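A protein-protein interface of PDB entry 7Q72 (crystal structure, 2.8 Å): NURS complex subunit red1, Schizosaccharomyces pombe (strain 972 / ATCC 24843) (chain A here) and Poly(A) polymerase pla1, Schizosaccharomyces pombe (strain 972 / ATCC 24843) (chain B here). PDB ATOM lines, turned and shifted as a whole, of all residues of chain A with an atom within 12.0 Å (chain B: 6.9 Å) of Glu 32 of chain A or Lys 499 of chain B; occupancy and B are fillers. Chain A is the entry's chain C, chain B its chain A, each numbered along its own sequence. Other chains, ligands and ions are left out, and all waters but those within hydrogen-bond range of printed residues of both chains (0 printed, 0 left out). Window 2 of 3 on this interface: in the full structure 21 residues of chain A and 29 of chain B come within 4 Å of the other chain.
Val 29 of chain A touches Leu 501 of chain B (CA to O, 3.3 Å).
CG1 of Val 30 of chain A touches CD2 of His 368 of chain B, at 3.5 Å.
CA of Arg 500 of chain B touches O of Val 30 of chain A, at 3.5 Å.
Ile 31 of chain A touches Lys 499 of chain B (CD1 to O, 3.5 Å).
Ile 498 of chain B touches Phe 33 of chain A (O to CD2, 3.1 Å).
The backbone NH (N) of Leu 501 of chain B sits at hydrogen-bond distance from the backbone carbonyl oxygen (O) of Val 30 of chain A (2.7 Å).
O of Lys 499 of chain B is in hydrogen-bond range of N of Glu 32 of chain A (3.0 Å).
OD1 of Asp 34 of chain A sits close to NE2 of His 368 of chain B (3.4 Å).
Hydrophobic or aromatic side chains of chain B that line the printed part of chain A: His 368, Ile 498 and Leu 501.
Of the 12 printed residues of chain A, 6 touch a printed residue of chain B.
Hydrophobic or aromatic side chains of chain A within 4 Å of the printed part of chain B: Val 29, Val 30, Ile 31 and Phe 33.
Among the printed residues, 8 pairs touch across the chains.
Among the printed residues, no Asp or Glu carboxylate lies within 4 Å of a Lys or Arg side-chain nitrogen of the other chain.
Printed residues of chain B within 4 Å of Val 29 of chain A: Leu 501 (3.3 Å).
Of the printed residues of chain B, Val 30 of chain A touches His 368, Arg 500 and Leu 501.
Of chain B, only Lys 499 (3.0 Å) comes within 4 Å of Glu 32 of chain A.
Printed residues of chain B within 4 Å of Phe 33 of chain A: Ile 498 (3.1 Å).
Ile 498 of chain B touches just one residue of chain A: Phe 33.
Lys 499 of chain B touches two residues of chain A.
The nearest residue of chain B that does not touch Glu 32 of chain A is Arg 500 of chain B (4.2 Å).
The nearest printed residue of chain A that does not touch Lys 499 of chain B is Val 30 of chain A (5.0 Å).
The nearest printed residue of chain B that does not touch Phe 33 of chain A is Leu 490 of chain B (5.0 Å).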
ATOM      1  N   ASN A  28      16.864  10.524   4.325  1.00  0.00           N
ATOM      2  CA  ASN A  28      16.448  11.918   4.362  1.00  0.00           C
ATOM      3  C   ASN A  28      14.977  12.059   3.993  1.00  0.00           C
ATOM      4  O   ASN A  28      14.379  11.179   3.368  1.00  0.00           O
ATOM      5  CB  ASN A  28      17.302  12.759   3.413  1.00  0.00           C
ATOM      6  CG  ASN A  28      18.780  12.627   3.694  1.00  0.00           C
ATOM      7  OD1 ASN A  28      19.249  11.576   4.130  1.00  0.00           O
ATOM      8  ND2 ASN A  28      19.524  13.698   3.453  1.00  0.00           N
ATOM      9  N   VAL A  29      14.398  13.194   4.383  1.00  0.00           N
ATOM     10  CA  VAL A  29      12.993  13.473   4.105  1.00  0.00           C
ATOM     11  C   VAL A  29      12.728  14.974   4.187  1.00  0.00           C
ATOM     12  O   VAL A  29      13.068  15.622   5.182  1.00  0.00           O
ATOM     13  CB  VAL A  29      12.081  12.691   5.070  1.00  0.00           C
ATOM     14  CG1 VAL A  29      12.599  12.792   6.506  1.00  0.00           C
ATOM     15  CG2 VAL A  29      10.653  13.192   4.976  1.00  0.00           C
ATOM     16  N   VAL A  30      12.123  15.537   3.139  1.00  0.00           N
ATOM     17  CA  VAL A  30      11.753  16.949   3.091  1.00  0.00           C
ATOM     18  C   VAL A  30      10.239  17.045   3.237  1.00  0.00           C
ATOM     19  O   VAL A  30       9.500  16.223   2.685  1.00  0.00           O
ATOM     20  CB  VAL A  30      12.232  17.618   1.788  1.00  0.00           C
ATOM     21  CG1 VAL A  30      11.853  19.085   1.770  1.00  0.00           C
ATOM     22  CG2 VAL A  30      13.739  17.459   1.625  1.00  0.00           C
ATOM     23  N   ILE A  31       9.775  18.046   3.982  1.00  0.00           N
ATOM     24  CA  ILE A  31       8.389  18.111   4.434  1.00  0.00           C
ATOM     25  C   ILE A  31       7.679  19.266   3.736  1.00  0.00           C
ATOM     26  O   ILE A  31       8.192  20.392   3.699  1.00  0.00           O
ATOM     27  CB  ILE A  31       8.315  18.235   5.970  1.00  0.00           C
ATOM     28  CG1 ILE A  31       6.998  18.865   6.437  1.00  0.00           C
ATOM     29  CG2 ILE A  31       9.509  19.001   6.522  1.00  0.00           C
ATOM     30  CD1 ILE A  31       5.793  17.941   6.345  1.00  0.00           C
ATOM     31  N   GLU A  32       6.507  18.971   3.165  1.00  0.00           N
ATOM     32  CA  GLU A  32       5.601  19.954   2.576  1.00  0.00           C
ATOM     33  C   GLU A  32       6.087  20.490   1.232  1.00  0.00           C
ATOM     34  O   GLU A  32       7.287  20.716   1.038  1.00  0.00           O
ATOM     35  CB  GLU A  32       5.368  21.132   3.533  1.00  0.00           C
ATOM     36  CG  GLU A  32       4.441  20.826   4.698  1.00  0.00           C
ATOM     37  CD  GLU A  32       3.997  22.072   5.453  1.00  0.00           C
ATOM     38  OE1 GLU A  32       2.868  22.071   5.987  1.00  0.00           O
ATOM     39  OE2 GLU A  32       4.772  23.050   5.516  1.00  0.00           O
ATOM     40  N   PHE A  33       5.152  20.701   0.301  1.00  0.00           N
ATOM     41  CA  PHE A  33       5.405  21.518  -0.878  1.00  0.00           C
ATOM     42  C   PHE A  33       5.197  23.004  -0.605  1.00  0.00           C
ATOM     43  O   PHE A  33       5.220  23.806  -1.548  1.00  0.00           O
ATOM     44  CB  PHE A  33       4.543  21.056  -2.067  1.00  0.00           C
ATOM     45  CG  PHE A  33       3.051  21.205  -1.869  1.00  0.00           C
ATOM     46  CD1 PHE A  33       2.392  22.343  -2.305  1.00  0.00           C
ATOM     47  CD2 PHE A  33       2.303  20.192  -1.284  1.00  0.00           C
ATOM     48  CE1 PHE A  33       1.027  22.481  -2.140  1.00  0.00           C
ATOM     49  CE2 PHE A  33       0.930  20.328  -1.114  1.00  0.00           C
ATOM     50  CZ  PHE A  33       0.295  21.475  -1.542  1.00  0.00           C
ATOM     51  N   ASP A  34       4.995  23.377   0.662  1.00  0.00           N
ATOM     52  CA  ASP A  34       5.046  24.769   1.117  1.00  0.00           C
ATOM     53  C   ASP A  34       3.936  25.619   0.499  1.00  0.00           C
ATOM     54  O   ASP A  34       4.179  26.684  -0.074  1.00  0.00           O
ATOM     55  CB  ASP A  34       6.426  25.378   0.856  1.00  0.00           C
ATOM     56  CG  ASP A  34       7.553  24.510   1.399  1.00  0.00           C
ATOM     57  OD1 ASP A  34       8.062  23.653   0.643  1.00  0.00           O
ATOM     58  OD2 ASP A  34       7.921  24.673   2.584  1.00  0.00           O
ATOM     59  N   SER A  35       2.700  25.134   0.625  1.00  0.00           N
ATOM     60  CA  SER A  35       1.527  25.968   0.394  1.00  0.00           C
ATOM     61  C   SER A  35       1.081  26.677   1.662  1.00  0.00           C
ATOM     62  O   SER A  35       0.458  27.743   1.586  1.00  0.00           O
ATOM     63  CB  SER A  35       0.368  25.129  -0.151  1.00  0.00           C
ATOM     64  OG  SER A  35      -0.760  25.943  -0.426  1.00  0.00           O
ATOM     65  N   ASP A  36       1.382  26.101   2.821  1.00  0.00           N
ATOM     66  CA  ASP A  36       1.212  26.754   4.107  1.00  0.00           C
ATOM     67  C   ASP A  36       2.580  27.151   4.648  1.00  0.00           C
ATOM     68  O   ASP A  36       3.582  26.474   4.397  1.00  0.00           O
ATOM     69  CB  ASP A  36       0.490  25.841   5.105  1.00  0.00           C
ATOM     70  CG  ASP A  36      -0.939  25.540   4.692  1.00  0.00           C
ATOM     71  OD1 ASP A  36      -1.606  26.447   4.148  1.00  0.00           O
ATOM     72  OD2 ASP A  36      -1.395  24.397   4.907  1.00  0.00           O
ATOM     73  N   ASP A  37       2.611  28.261   5.388  1.00  0.00           N
ATOM     74  CA  ASP A  37       3.857  28.858   5.875  1.00  0.00           C
ATOM     75  C   ASP A  37       4.786  29.208   4.712  1.00  0.00           C
ATOM     76  O   ASP A  37       5.948  28.799   4.667  1.00  0.00           O
ATOM     77  CB  ASP A  37       4.562  27.942   6.883  1.00  0.00           C
ATOM     78  CG  ASP A  37       3.815  27.834   8.202  1.00  0.00           C
ATOM     79  OD1 ASP A  37       3.153  28.818   8.598  1.00  0.00           O
ATOM     80  OD2 ASP A  37       3.899  26.764   8.845  1.00  0.00           O
ATOM     81  N   ASP A  38       4.257  29.975   3.761  1.00  0.00           N
ATOM     82  CA  ASP A  38       5.040  30.398   2.610  1.00  0.00           C
ATOM     83  C   ASP A  38       6.083  31.437   3.019  1.00  0.00           C
ATOM     84  O   ASP A  38       6.111  31.928   4.152  1.00  0.00           O
ATOM     85  CB  ASP A  38       4.132  30.967   1.519  1.00  0.00           C
ATOM     86  CG  ASP A  38       3.550  29.890   0.625  1.00  0.00           C
ATOM     87  OD1 ASP A  38       2.972  28.924   1.161  1.00  0.00           O
ATOM     88  OD2 ASP A  38       3.663  30.014  -0.614  1.00  0.00           O
ATOM     89  N   GLY A  39       6.951  31.771   2.069  1.00  0.00           N
ATOM     90  CA  GLY A  39       7.983  32.765   2.294  1.00  0.00           C
ATOM     91  C   GLY A  39       7.484  34.192   2.162  1.00  0.00           C
ATOM     92  O   GLY A  39       6.431  34.441   1.571  1.00  0.00           O
ATOM     93  N   HIS B 368      15.007  24.862  -0.763  1.00  0.00           N
ATOM     94  CA  HIS B 368      15.570  23.726  -0.047  1.00  0.00           C
ATOM     95  C   HIS B 368      16.937  23.390  -0.623  1.00  0.00           C
ATOM     96  O   HIS B 368      17.082  23.245  -1.841  1.00  0.00           O
ATOM     97  CB  HIS B 368      14.641  22.511  -0.130  1.00  0.00           C
ATOM     98  CG  HIS B 368      13.246  22.789   0.332  1.00  0.00           C
ATOM     99  ND1 HIS B 368      12.315  23.428  -0.457  1.00  0.00           N
ATOM    100  CD2 HIS B 368      12.627  22.526   1.507  1.00  0.00           C
ATOM    101  CE1 HIS B 368      11.180  23.541   0.209  1.00  0.00           C
ATOM    102  NE2 HIS B 368      11.343  23.002   1.405  1.00  0.00           N
ATOM    103  N   LEU B 490      11.197  22.358  -6.471  1.00  0.00           N
ATOM    104  CA  LEU B 490      10.257  21.253  -6.337  1.00  0.00           C
ATOM    105  C   LEU B 490       9.117  21.363  -7.343  1.00  0.00           C
ATOM    106  O   LEU B 490       8.601  22.454  -7.602  1.00  0.00           O
ATOM    107  CB  LEU B 490       9.698  21.201  -4.916  1.00  0.00           C
ATOM    108  CG  LEU B 490      10.751  20.994  -3.826  1.00  0.00           C
ATOM    109  CD1 LEU B 490      10.093  20.790  -2.469  1.00  0.00           C
ATOM    110  CD2 LEU B 490      11.658  19.821  -4.172  1.00  0.00           C
ATOM    111  N   ILE B 498       3.139  14.726  -1.898  1.00  0.00           N
ATOM    112  CA  ILE B 498       2.345  15.907  -1.578  1.00  0.00           C
ATOM    113  C   ILE B 498       2.642  16.379  -0.157  1.00  0.00           C
ATOM    114  O   ILE B 498       3.110  17.499   0.049  1.00  0.00           O
ATOM    115  CB  ILE B 498       0.840  15.631  -1.761  1.00  0.00           C
ATOM    116  CG1 ILE B 498       0.530  15.331  -3.230  1.00  0.00           C
ATOM    117  CG2 ILE B 498       0.015  16.810  -1.267  1.00  0.00           C
ATOM    118  CD1 ILE B 498      -0.942  15.116  -3.513  1.00  0.00           C
ATOM    119  N   LYS B 499       2.372  15.515   0.824  1.00  0.00           N
ATOM    120  CA  LYS B 499       2.597  15.891   2.217  1.00  0.00           C
ATOM    121  C   LYS B 499       4.083  15.893   2.558  1.00  0.00           C
ATOM    122  O   LYS B 499       4.546  16.740   3.331  1.00  0.00           O
ATOM    123  CB  LYS B 499       1.832  14.949   3.146  1.00  0.00           C
ATOM    124  CG  LYS B 499       0.319  15.019   2.996  1.00  0.00           C
ATOM    125  CD  LYS B 499      -0.376  14.046   3.936  1.00  0.00           C
ATOM    126  CE  LYS B 499      -1.889  14.108   3.780  1.00  0.00           C
ATOM    127  NZ  LYS B 499      -2.582  13.140   4.675  1.00  0.00           N
ATOM    128  N   ARG B 500       4.844  14.957   1.995  1.00  0.00           N
ATOM    129  CA  ARG B 500       6.272  14.864   2.265  1.00  0.00           C
ATOM    130  C   ARG B 500       6.977  14.320   1.031  1.00  0.00           C
ATOM    131  O   ARG B 500       6.346  13.839   0.087  1.00  0.00           O
ATOM    132  CB  ARG B 500       6.555  13.981   3.486  1.00  0.00           C
ATOM    133  CG  ARG B 500       6.048  12.555   3.345  1.00  0.00           C
ATOM    134  CD  ARG B 500       6.469  11.690   4.522  1.00  0.00           C
ATOM    135  NE  ARG B 500       5.979  10.323   4.390  1.00  0.00           N
ATOM    136  CZ  ARG B 500       6.613   9.360   3.734  1.00  0.00           C
ATOM    137  NH1 ARG B 500       7.774   9.578   3.137  1.00  0.00           N
ATOM    138  NH2 ARG B 500       6.069   8.148   3.676  1.00  0.00           N
ATOM    139  N   LEU B 501       8.305  14.403   1.052  1.00  0.00           N
ATOM    140  CA  LEU B 501       9.149  13.895  -0.020  1.00  0.00           C
ATOM    141  C   LEU B 501      10.231  13.007   0.573  1.00  0.00           C
ATOM    142  O   LEU B 501      10.849  13.360   1.582  1.00  0.00           O
ATOM    143  CB  LEU B 501       9.787  15.035  -0.819  1.00  0.00           C
ATOM    144  CG  LEU B 501      10.794  14.625  -1.894  1.00  0.00           C
ATOM    145  CD1 LEU B 501      10.143  13.708  -2.917  1.00  0.00           C
ATOM    146  CD2 LEU B 501      11.389  15.849  -2.569  1.00  0.00           C
ATOM    147  N   LYS B 533      16.682  24.326   4.976  1.00  0.00           N
ATOM    148  CA  LYS B 533      15.761  25.302   4.420  1.00  0.00           C
ATOM    149  C   LYS B 533      16.487  26.627   4.189  1.00  0.00           C
ATOM    150  O   LYS B 533      17.674  26.773   4.484  1.00  0.00           O
ATOM    151  CB  LYS B 533      14.558  25.483   5.346  1.00  0.00           C
ATOM    152  CG  LYS B 533      13.813  24.194   5.652  1.00  0.00           C
ATOM    153  CD  LYS B 533      12.659  24.433   6.615  1.00  0.00           C
ATOM    154  CE  LYS B 533      11.944  23.134   6.954  1.00  0.00           C
ATOM    155  NZ  LYS B 533      10.809  23.352   7.894  1.00  0.00           N
